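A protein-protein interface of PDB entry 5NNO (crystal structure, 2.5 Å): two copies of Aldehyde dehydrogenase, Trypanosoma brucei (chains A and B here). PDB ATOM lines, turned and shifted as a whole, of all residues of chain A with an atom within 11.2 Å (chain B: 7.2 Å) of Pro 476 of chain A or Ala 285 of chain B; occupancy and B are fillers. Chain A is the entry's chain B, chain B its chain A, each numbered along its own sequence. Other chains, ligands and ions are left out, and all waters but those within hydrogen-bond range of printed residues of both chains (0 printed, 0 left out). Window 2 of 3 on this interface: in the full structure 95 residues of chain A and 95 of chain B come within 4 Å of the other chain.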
ATOM      1  N   ASP A 470      17.992 -29.451  24.788  1.00  0.00           N
ATOM      2  CA  ASP A 470      19.416 -29.502  25.171  1.00  0.00           C
ATOM      3  C   ASP A 470      20.406 -29.479  24.000  1.00  0.00           C
ATOM      4  O   ASP A 470      21.598 -29.245  24.224  1.00  0.00           O
ATOM      5  CB  ASP A 470      19.706 -30.731  26.053  1.00  0.00           C
ATOM      6  CG  ASP A 470      19.115 -30.615  27.450  1.00  0.00           C
ATOM      7  OD1 ASP A 470      19.021 -29.490  27.990  1.00  0.00           O
ATOM      8  OD2 ASP A 470      18.763 -31.668  28.022  1.00  0.00           O
ATOM      9  N   THR A 471      19.928 -29.718  22.774  1.00  0.00           N
ATOM     10  CA  THR A 471      20.763 -29.621  21.569  1.00  0.00           C
ATOM     11  C   THR A 471      21.223 -28.204  21.241  1.00  0.00           C
ATOM     12  O   THR A 471      22.215 -28.050  20.533  1.00  0.00           O
ATOM     13  CB  THR A 471      20.047 -30.176  20.313  1.00  0.00           C
ATOM     14  OG1 THR A 471      18.758 -29.566  20.178  1.00  0.00           O
ATOM     15  CG2 THR A 471      19.878 -31.680  20.413  1.00  0.00           C
ATOM     16  N   VAL A 472      20.510 -27.183  21.731  1.00  0.00           N
ATOM     17  CA  VAL A 472      20.787 -25.788  21.345  1.00  0.00           C
ATOM     18  C   VAL A 472      21.012 -24.764  22.465  1.00  0.00           C
ATOM     19  O   VAL A 472      21.549 -23.684  22.185  1.00  0.00           O
ATOM     20  CB  VAL A 472      19.713 -25.236  20.369  1.00  0.00           C
ATOM     21  CG1 VAL A 472      19.753 -26.007  19.051  1.00  0.00           C
ATOM     22  CG2 VAL A 472      18.314 -25.272  20.988  1.00  0.00           C
ATOM     23  N   ARG A 473      20.650 -25.076  23.712  1.00  0.00           N
ATOM     24  CA  ARG A 473      20.662 -24.050  24.759  1.00  0.00           C
ATOM     25  C   ARG A 473      22.048 -23.740  25.356  1.00  0.00           C
ATOM     26  O   ARG A 473      22.428 -22.576  25.445  1.00  0.00           O
ATOM     27  CB  ARG A 473      19.613 -24.343  25.848  1.00  0.00           C
ATOM     28  CG  ARG A 473      19.882 -25.499  26.801  1.00  0.00           C
ATOM     29  CD  ARG A 473      19.004 -25.380  28.037  1.00  0.00           C
ATOM     30  NE  ARG A 473      18.518 -26.659  28.542  1.00  0.00           N
ATOM     31  CZ  ARG A 473      17.798 -26.799  29.650  1.00  0.00           C
ATOM     32  NH1 ARG A 473      17.462 -25.733  30.369  1.00  0.00           N
ATOM     33  NH2 ARG A 473      17.386 -28.005  30.033  1.00  0.00           N
ATOM     34  N   PHE A 474      22.816 -24.770  25.721  1.00  0.00           N
ATOM     35  CA  PHE A 474      24.013 -24.572  26.560  1.00  0.00           C
ATOM     36  C   PHE A 474      25.225 -24.033  25.789  1.00  0.00           C
ATOM     37  O   PHE A 474      25.619 -24.618  24.786  1.00  0.00           O
ATOM     38  CB  PHE A 474      24.376 -25.867  27.279  1.00  0.00           C
ATOM     39  CG  PHE A 474      23.302 -26.367  28.208  1.00  0.00           C
ATOM     40  CD1 PHE A 474      22.945 -25.639  29.347  1.00  0.00           C
ATOM     41  CD2 PHE A 474      22.642 -27.564  27.954  1.00  0.00           C
ATOM     42  CE1 PHE A 474      21.948 -26.095  30.212  1.00  0.00           C
ATOM     43  CE2 PHE A 474      21.649 -28.022  28.819  1.00  0.00           C
ATOM     44  CZ  PHE A 474      21.295 -27.284  29.945  1.00  0.00           C
ATOM     45  N   PRO A 475      25.812 -22.905  26.244  1.00  0.00           N
ATOM     46  CA  PRO A 475      27.100 -22.495  25.662  1.00  0.00           C
ATOM     47  C   PRO A 475      28.254 -23.469  26.053  1.00  0.00           C
ATOM     48  O   PRO A 475      28.074 -24.269  26.977  1.00  0.00           O
ATOM     49  CB  PRO A 475      27.323 -21.081  26.223  1.00  0.00           C
ATOM     50  CG  PRO A 475      26.078 -20.695  26.921  1.00  0.00           C
ATOM     51  CD  PRO A 475      25.303 -21.926  27.217  1.00  0.00           C
ATOM     52  N   PRO A 476      29.426 -23.409  25.412  1.00  0.00           N
ATOM     53  CA  PRO A 476      29.837 -22.360  24.484  1.00  0.00           C
ATOM     54  C   PRO A 476      29.134 -22.416  23.141  1.00  0.00           C
ATOM     55  O   PRO A 476      28.627 -23.470  22.745  1.00  0.00           O
ATOM     56  CB  PRO A 476      31.325 -22.669  24.283  1.00  0.00           C
ATOM     57  CG  PRO A 476      31.389 -24.158  24.364  1.00  0.00           C
ATOM     58  CD  PRO A 476      30.291 -24.603  25.295  1.00  0.00           C
ATOM     59  N   TYR A 477      29.135 -21.279  22.455  1.00  0.00           N
ATOM     60  CA  TYR A 477      28.451 -21.119  21.173  1.00  0.00           C
ATOM     61  C   TYR A 477      29.350 -21.575  20.018  1.00  0.00           C
ATOM     62  O   TYR A 477      30.010 -20.777  19.356  1.00  0.00           O
ATOM     63  CB  TYR A 477      27.958 -19.665  21.014  1.00  0.00           C
ATOM     64  CG  TYR A 477      26.926 -19.298  22.072  1.00  0.00           C
ATOM     65  CD1 TYR A 477      25.734 -20.020  22.173  1.00  0.00           C
ATOM     66  CD2 TYR A 477      27.140 -18.259  22.986  1.00  0.00           C
ATOM     67  CE1 TYR A 477      24.780 -19.720  23.134  1.00  0.00           C
ATOM     68  CE2 TYR A 477      26.194 -17.964  23.959  1.00  0.00           C
ATOM     69  CZ  TYR A 477      25.013 -18.697  24.023  1.00  0.00           C
ATOM     70  OH  TYR A 477      24.046 -18.434  24.965  1.00  0.00           O
ATOM     71  N   THR A 478      29.354 -22.888  19.789  1.00  0.00           N
ATOM     72  CA  THR A 478      30.204 -23.516  18.774  1.00  0.00           C
ATOM     73  C   THR A 478      29.677 -23.211  17.367  1.00  0.00           C
ATOM     74  O   THR A 478      28.542 -22.746  17.214  1.00  0.00           O
ATOM     75  CB  THR A 478      30.305 -25.047  18.994  1.00  0.00           C
ATOM     76  OG1 THR A 478      28.999 -25.633  18.969  1.00  0.00           O
ATOM     77  CG2 THR A 478      30.964 -25.366  20.328  1.00  0.00           C
ATOM     78  N   THR A 479      30.516 -23.443  16.351  1.00  0.00           N
ATOM     79  CA  THR A 479      30.101 -23.334  14.941  1.00  0.00           C
ATOM     80  C   THR A 479      29.081 -24.424  14.595  1.00  0.00           C
ATOM     81  O   THR A 479      28.182 -24.213  13.785  1.00  0.00           O
ATOM     82  CB  THR A 479      31.293 -23.478  13.964  1.00  0.00           C
ATOM     83  OG1 THR A 479      32.374 -22.622  14.355  1.00  0.00           O
ATOM     84  CG2 THR A 479      30.892 -23.121  12.531  1.00  0.00           C
ATOM     85  N   ALA A 480      29.253 -25.597  15.199  1.00  0.00           N
ATOM     86  CA  ALA A 480      28.300 -26.706  15.054  1.00  0.00           C
ATOM     87  C   ALA A 480      26.909 -26.374  15.634  1.00  0.00           C
ATOM     88  O   ALA A 480      25.897 -26.804  15.086  1.00  0.00           O
ATOM     89  CB  ALA A 480      28.863 -27.970  15.695  1.00  0.00           C
ATOM     90  N   LYS A 481      26.877 -25.621  16.735  1.00  0.00           N
ATOM     91  CA  LYS A 481      25.628 -25.134  17.339  1.00  0.00           C
ATOM     92  C   LYS A 481      24.937 -24.076  16.457  1.00  0.00           C
ATOM     93  O   LYS A 481      23.705 -24.026  16.385  1.00  0.00           O
ATOM     94  CB  LYS A 481      25.910 -24.588  18.750  1.00  0.00           C
ATOM     95  CG  LYS A 481      24.697 -24.025  19.493  1.00  0.00           C
ATOM     96  CD  LYS A 481      24.791 -24.168  21.013  1.00  0.00           C
ATOM     97  CE  LYS A 481      24.508 -25.592  21.440  1.00  0.00           C
ATOM     98  NZ  LYS A 481      24.214 -25.760  22.884  1.00  0.00           N
ATOM     99  N   SER A 482      25.734 -23.240  15.789  1.00  0.00           N
ATOM    100  CA  SER A 482      25.226 -22.233  14.849  1.00  0.00           C
ATOM    101  C   SER A 482      24.593 -22.840  13.585  1.00  0.00           C
ATOM    102  O   SER A 482      23.535 -22.372  13.123  1.00  0.00           O
ATOM    103  CB  SER A 482      26.352 -21.281  14.456  1.00  0.00           C
ATOM    104  OG  SER A 482      26.895 -20.650  15.605  1.00  0.00           O
ATOM    105  N   ARG A 483      25.240 -23.872  13.036  1.00  0.00           N
ATOM    106  CA  ARG A 483      24.739 -24.555  11.823  1.00  0.00           C
ATOM    107  C   ARG A 483      23.431 -25.327  12.069  1.00  0.00           C
ATOM    108  O   ARG A 483      22.605 -25.415  11.164  1.00  0.00           O
ATOM    109  CB  ARG A 483      25.819 -25.464  11.180  1.00  0.00           C
ATOM    110  CG  ARG A 483      26.485 -24.888   9.920  1.00  0.00           C
ATOM    111  CD  ARG A 483      28.009 -25.004   9.932  1.00  0.00           C
ATOM    112  NE  ARG A 483      28.633 -24.415   8.739  1.00  0.00           N
ATOM    113  CZ  ARG A 483      29.944 -24.403   8.472  1.00  0.00           C
ATOM    114  NH1 ARG A 483      30.826 -24.947   9.304  1.00  0.00           N
ATOM    115  NH2 ARG A 483      30.385 -23.838   7.348  1.00  0.00           N
ATOM    116  N   VAL A 484      23.246 -25.859  13.282  1.00  0.00           N
ATOM    117  CA  VAL A 484      21.964 -26.477  13.733  1.00  0.00           C
ATOM    118  C   VAL A 484      20.814 -25.443  13.832  1.00  0.00           C
ATOM    119  O   VAL A 484      19.684 -25.726  13.422  1.00  0.00           O
ATOM    120  CB  VAL A 484      22.128 -27.219  15.098  1.00  0.00           C
ATOM    121  CG1 VAL A 484      20.794 -27.714  15.662  1.00  0.00           C
ATOM    122  CG2 VAL A 484      23.085 -28.405  14.955  1.00  0.00           C
ATOM    123  N   LEU A 485      21.112 -24.271  14.392  1.00  0.00           N
ATOM    124  CA  LEU A 485      20.128 -23.195  14.548  1.00  0.00           C
ATOM    125  C   LEU A 485      19.818 -22.487  13.238  1.00  0.00           C
ATOM    126  O   LEU A 485      18.675 -22.079  13.012  1.00  0.00           O
ATOM    127  CB  LEU A 485      20.608 -22.163  15.573  1.00  0.00           C
ATOM    128  CG  LEU A 485      20.677 -22.623  17.020  1.00  0.00           C
ATOM    129  CD1 LEU A 485      21.329 -21.551  17.881  1.00  0.00           C
ATOM    130  CD2 LEU A 485      19.278 -22.946  17.526  1.00  0.00           C
ATOM    131  N   ASP B  70      23.383 -16.846  18.451  1.00  0.00           N
ATOM    132  CA  ASP B  70      22.724 -18.093  18.843  1.00  0.00           C
ATOM    133  C   ASP B  70      21.927 -17.958  20.140  1.00  0.00           C
ATOM    134  O   ASP B  70      20.887 -18.594  20.272  1.00  0.00           O
ATOM    135  CB  ASP B  70      23.747 -19.227  18.987  1.00  0.00           C
ATOM    136  CG  ASP B  70      24.437 -19.563  17.679  1.00  0.00           C
ATOM    137  OD1 ASP B  70      24.280 -18.798  16.706  1.00  0.00           O
ATOM    138  OD2 ASP B  70      25.164 -20.574  17.638  1.00  0.00           O
ATOM    139  N   LYS B 241      25.132 -32.639  38.262  1.00  0.00           N
ATOM    140  CA  LYS B 241      25.663 -31.996  37.047  1.00  0.00           C
ATOM    141  C   LYS B 241      24.562 -31.403  36.147  1.00  0.00           C
ATOM    142  O   LYS B 241      24.775 -30.377  35.507  1.00  0.00           O
ATOM    143  CB  LYS B 241      26.550 -32.990  36.284  1.00  0.00           C
ATOM    144  CG  LYS B 241      27.216 -32.445  35.016  1.00  0.00           C
ATOM    145  CD  LYS B 241      28.373 -33.375  34.660  1.00  0.00           C
ATOM    146  CE  LYS B 241      29.250 -32.906  33.490  1.00  0.00           C
ATOM    147  NZ  LYS B 241      28.485 -32.288  32.347  1.00  0.00           N
ATOM    148  N   GLU B 245      24.176 -27.322  35.711  1.00  0.00           N
ATOM    149  CA  GLU B 245      24.241 -26.769  34.349  1.00  0.00           C
ATOM    150  C   GLU B 245      22.960 -26.020  33.964  1.00  0.00           C
ATOM    151  O   GLU B 245      23.014 -25.030  33.238  1.00  0.00           O
ATOM    152  CB  GLU B 245      24.537 -27.869  33.321  1.00  0.00           C
ATOM    153  CG  GLU B 245      25.938 -28.442  33.440  1.00  0.00           C
ATOM    154  CD  GLU B 245      26.131 -29.734  32.641  1.00  0.00           C
ATOM    155  OE1 GLU B 245      25.184 -30.563  32.579  1.00  0.00           O
ATOM    156  OE2 GLU B 245      27.234 -29.920  32.062  1.00  0.00           O
ATOM    157  N   ILE B 252      23.766 -17.349  33.354  1.00  0.00           N
ATOM    158  CA  ILE B 252      24.777 -16.853  32.394  1.00  0.00           C
ATOM    159  C   ILE B 252      24.116 -16.010  31.306  1.00  0.00           C
ATOM    160  O   ILE B 252      24.615 -14.928  30.970  1.00  0.00           O
ATOM    161  CB  ILE B 252      25.646 -18.006  31.781  1.00  0.00           C
ATOM    162  CG1 ILE B 252      26.768 -18.370  32.754  1.00  0.00           C
ATOM    163  CG2 ILE B 252      26.269 -17.591  30.445  1.00  0.00           C
ATOM    164  CD1 ILE B 252      27.544 -19.624  32.419  1.00  0.00           C
ATOM    165  N   LEU B 279      28.133 -26.046  40.186  1.00  0.00           N
ATOM    166  CA  LEU B 279      27.965 -24.747  39.529  1.00  0.00           C
ATOM    167  C   LEU B 279      29.264 -24.158  38.963  1.00  0.00           C
ATOM    168  O   LEU B 279      29.253 -23.607  37.873  1.00  0.00           O
ATOM    169  CB  LEU B 279      27.292 -23.748  40.477  1.00  0.00           C
ATOM    170  CG  LEU B 279      25.827 -24.065  40.833  1.00  0.00           C
ATOM    171  CD1 LEU B 279      25.507 -23.498  42.196  1.00  0.00           C
ATOM    172  CD2 LEU B 279      24.849 -23.544  39.776  1.00  0.00           C
ATOM    173  N   ALA B 280      30.370 -24.268  39.701  1.00  0.00           N
ATOM    174  CA  ALA B 280      31.696 -23.788  39.234  1.00  0.00           C
ATOM    175  C   ALA B 280      32.238 -24.509  37.984  1.00  0.00           C
ATOM    176  O   ALA B 280      32.764 -23.854  37.075  1.00  0.00           O
ATOM    177  CB  ALA B 280      32.712 -23.898  40.349  1.00  0.00           C
ATOM    178  N   GLU B 281      32.135 -25.842  37.957  1.00  0.00           N
ATOM    179  CA  GLU B 281      32.427 -26.626  36.751  1.00  0.00           C
ATOM    180  C   GLU B 281      31.470 -26.309  35.555  1.00  0.00           C
ATOM    181  O   GLU B 281      31.917 -26.235  34.398  1.00  0.00           O
ATOM    182  CB  GLU B 281      32.475 -28.137  37.051  1.00  0.00           C
ATOM    183  CG  GLU B 281      33.628 -28.561  37.976  1.00  0.00           C
ATOM    184  CD  GLU B 281      35.028 -28.393  37.349  1.00  0.00           C
ATOM    185  OE1 GLU B 281      35.389 -29.144  36.419  1.00  0.00           O
ATOM    186  OE2 GLU B 281      35.786 -27.509  37.797  1.00  0.00           O
ATOM    187  N   ALA B 282      30.180 -26.136  35.838  1.00  0.00           N
ATOM    188  CA  ALA B 282      29.205 -25.685  34.821  1.00  0.00           C
ATOM    189  C   ALA B 282      29.589 -24.318  34.233  1.00  0.00           C
ATOM    190  O   ALA B 282      29.559 -24.113  33.024  1.00  0.00           O
ATOM    191  CB  ALA B 282      27.788 -25.615  35.422  1.00  0.00           C
ATOM    192  N   ARG B 283      29.934 -23.392  35.125  1.00  0.00           N
ATOM    193  CA  ARG B 283      30.390 -22.049  34.764  1.00  0.00           C
ATOM    194  C   ARG B 283      31.594 -22.064  33.854  1.00  0.00           C
ATOM    195  O   ARG B 283      31.608 -21.392  32.827  1.00  0.00           O
ATOM    196  CB  ARG B 283      30.737 -21.256  36.028  1.00  0.00           C
ATOM    197  CG  ARG B 283      30.985 -19.770  35.821  1.00  0.00           C
ATOM    198  CD  ARG B 283      31.201 -19.126  37.192  1.00  0.00           C
ATOM    199  NE  ARG B 283      31.737 -17.778  37.204  1.00  0.00           N
ATOM    200  CZ  ARG B 283      33.018 -17.417  37.253  1.00  0.00           C
ATOM    201  NH1 ARG B 283      34.022 -18.267  37.289  1.00  0.00           N
ATOM    202  NH2 ARG B 283      33.280 -16.136  37.317  1.00  0.00           N
ATOM    203  N   LYS B 284      32.603 -22.851  34.233  1.00  0.00           N
ATOM    204  CA  LYS B 284      33.837 -22.965  33.462  1.00  0.00           C
ATOM    205  C   LYS B 284      33.589 -23.538  32.080  1.00  0.00           C
ATOM    206  O   LYS B 284      34.108 -23.021  31.104  1.00  0.00           O
ATOM    207  CB  LYS B 284      34.910 -23.763  34.232  1.00  0.00           C
ATOM    208  CG  LYS B 284      35.636 -22.896  35.270  1.00  0.00           C
ATOM    209  CD  LYS B 284      36.942 -23.511  35.801  1.00  0.00           C
ATOM    210  CE  LYS B 284      36.750 -24.026  37.214  1.00  0.00           C
ATOM    211  NZ  LYS B 284      37.990 -24.732  37.700  1.00  0.00           N
ATOM    212  N   ALA B 285      32.768 -24.584  32.016  1.00  0.00           N
ATOM    213  CA  ALA B 285      32.359 -25.196  30.743  1.00  0.00           C
ATOM    214  C   ALA B 285      31.688 -24.211  29.768  1.00  0.00           C
ATOM    215  O   ALA B 285      31.986 -24.224  28.583  1.00  0.00           O
ATOM    216  CB  ALA B 285      31.439 -26.384  31.003  1.00  0.00           C
ATOM    217  N   MET B 286      30.833 -23.335  30.297  1.00  0.00           N
ATOM    218  CA  MET B 286      29.954 -22.454  29.503  1.00  0.00           C
ATOM    219  C   MET B 286      30.607 -21.117  29.107  1.00  0.00           C
ATOM    220  O   MET B 286      30.259 -20.535  28.072  1.00  0.00           O
ATOM    221  CB  MET B 286      28.630 -22.178  30.253  1.00  0.00           C
ATOM    222  CG  MET B 286      27.677 -23.353  30.327  1.00  0.00           C
ATOM    223  SD  MET B 286      26.162 -23.053  31.265  1.00  0.00           S
ATOM    224  CE  MET B 286      25.495 -24.712  31.317  1.00  0.00           C
ATOM    225  N   LEU B 287      31.490 -20.605  29.955  1.00  0.00           N
ATOM    226  CA  LEU B 287      32.194 -19.350  29.691  1.00  0.00           C
ATOM    227  C   LEU B 287      33.571 -19.560  29.043  1.00  0.00           C
ATOM    228  O   LEU B 287      34.140 -18.638  28.470  1.00  0.00           O
ATOM    229  CB  LEU B 287      32.349 -18.549  30.990  1.00  0.00           C
ATOM    230  CG  LEU B 287      31.051 -18.307  31.790  1.00  0.00           C
ATOM    231  CD1 LEU B 287      31.352 -17.755  33.173  1.00  0.00           C
ATOM    232  CD2 LEU B 287      30.112 -17.391  31.031  1.00  0.00           C
ATOM    233  N   GLY B 288      34.124 -20.757  29.171  1.00  0.00           N
ATOM    234  CA  GLY B 288      35.367 -21.081  28.513  1.00  0.00           C
ATOM    235  C   GLY B 288      36.600 -20.528  29.213  1.00  0.00           C
ATOM    236  O   GLY B 288      36.587 -19.429  29.780  1.00  0.00           O
ATOM    237  N   ASP B 289      37.682 -21.299  29.104  1.00  0.00           N
ATOM    238  CA  ASP B 289      38.945 -21.059  29.828  1.00  0.00           C
ATOM    239  C   ASP B 289      39.641 -19.712  29.573  1.00  0.00           C
ATOM    240  O   ASP B 289      39.870 -18.935  30.513  1.00  0.00           O
ATOM    241  CB  ASP B 289      39.909 -22.196  29.535  1.00  0.00           C
ATOM    242  CG  ASP B 289      41.059 -22.258  30.524  1.00  0.00           C
ATOM    243  OD1 ASP B 289      40.756 -22.375  31.745  1.00  0.00           O
ATOM    244  OD2 ASP B 289      42.239 -22.177  30.073  1.00  0.00           O
ATOM    245  N   LEU B 292      37.806 -16.488  31.128  1.00  0.00           N
ATOM    246  CA  LEU B 292      37.899 -16.283  32.576  1.00  0.00           C
ATOM    247  C   LEU B 292      39.300 -15.953  33.048  1.00  0.00           C
ATOM    248  O   LEU B 292      39.477 -15.199  34.023  1.00  0.00           O
ATOM    249  CB  LEU B 292      37.345 -17.496  33.350  1.00  0.00           C
ATOM    250  CG  LEU B 292      35.804 -17.685  33.345  1.00  0.00           C
ATOM    251  CD1 LEU B 292      35.438 -18.934  34.138  1.00  0.00           C
ATOM    252  CD2 LEU B 292      35.024 -16.496  33.917  1.00  0.00           C
ATOM    253  N   ASP B 312      31.850 -13.878  23.888  1.00  0.00           N
ATOM    254  CA  ASP B 312      30.499 -14.457  23.914  1.00  0.00           C
ATOM    255  C   ASP B 312      29.647 -14.077  25.123  1.00  0.00           C
ATOM    256  O   ASP B 312      28.436 -14.307  25.113  1.00  0.00           O
ATOM    257  CB  ASP B 312      30.587 -15.992  23.889  1.00  0.00           C
ATOM    258  CG  ASP B 312      31.180 -16.531  22.609  1.00  0.00           C
ATOM    259  OD1 ASP B 312      31.373 -15.776  21.634  1.00  0.00           O
ATOM    260  OD2 ASP B 312      31.433 -17.743  22.579  1.00  0.00           O
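Among the printed residues, pairs that only touch across the chains: Phe 474 of chain A with Met 286 of chain B (3.4 Å), Phe 474 of chain A with Glu 245 of chain B (3.4 Å), Pro 475 of chain A with Met 286 of chain B (3.5 Å), Leu 485 of chain A with Asp 70 of chain B (3.5 Å), Lys 481 of chain A with Asp 70 of chain B (3.7 Å), Pro 476 of chain A with Ala 285 of chain B (3.7 Å) and Tyr 477 of chain A with Asp 70 of chain B (3.8 Å).
O of Thr 478 of chain A lies within hydrogen-bond range of OG of Ser 482 of chain A (3.1 Å). The backbone carbonyl oxygen (O) of Val 472 of chain A sits close to the side-chain amino group (NZ) of Lys 481 of chain A (3.4 Å). OG1 of Thr 478 of chain A sits at hydrogen-bond distance from N of Lys 481 of chain A (3.1 Å). NZ of Lys 241 of chain B lies within salt-bridge range of OE2 of Glu 245 of chain B, 2.7 Å away. NZ of Lys 481 of chain A lies within hydrogen-bond range of O of Phe 474 of chain A (2.6 Å).
OG of Ser 482 of chain A sits at hydrogen-bond distance from OD2 of Asp 70 of chain B (2.7 Å).
No position is printed for both chains. Of the 8 pairs that touch across the chains among the printed residues, none has its exchanged pair printed and touching as well.
Hydrophobic or aromatic side chains of chain A that line the printed part of chain B: Phe 474, Pro 475, Pro 476, Tyr 477 and Leu 485. Hydrophobic or aromatic side chains of chain B that line the printed part of chain A: Met 286.
Printed residues of chain B within 4 Å of Pro 476 of chain A: Ala 285 (3.7 Å). Ala 285 of chain B touches just one residue of chain A: Pro 476 (3.7 Å). No residue of chain A comes within 4 Å of Ala 282 of chain B. Of the printed residues of chain B, Pro 475 of chain A touches Met 286 (3.5 Å). Printed residues of chain B within 4 Å of Ser 482 of chain A: Asp 70 (2.7 Å). Of the printed residues of chain A, Glu 245 of chain B touches Phe 474 (3.4 Å). Printed residues of chain B within 4 Å of Tyr 477 of chain A: Asp 70 (3.8 Å). Of the printed residues of chain B, Leu 485 of chain A touches Asp 70. The nearest printed residue of chain B that does not touch Pro 476 of chain A is Met 286 of chain B (4.004 Å).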
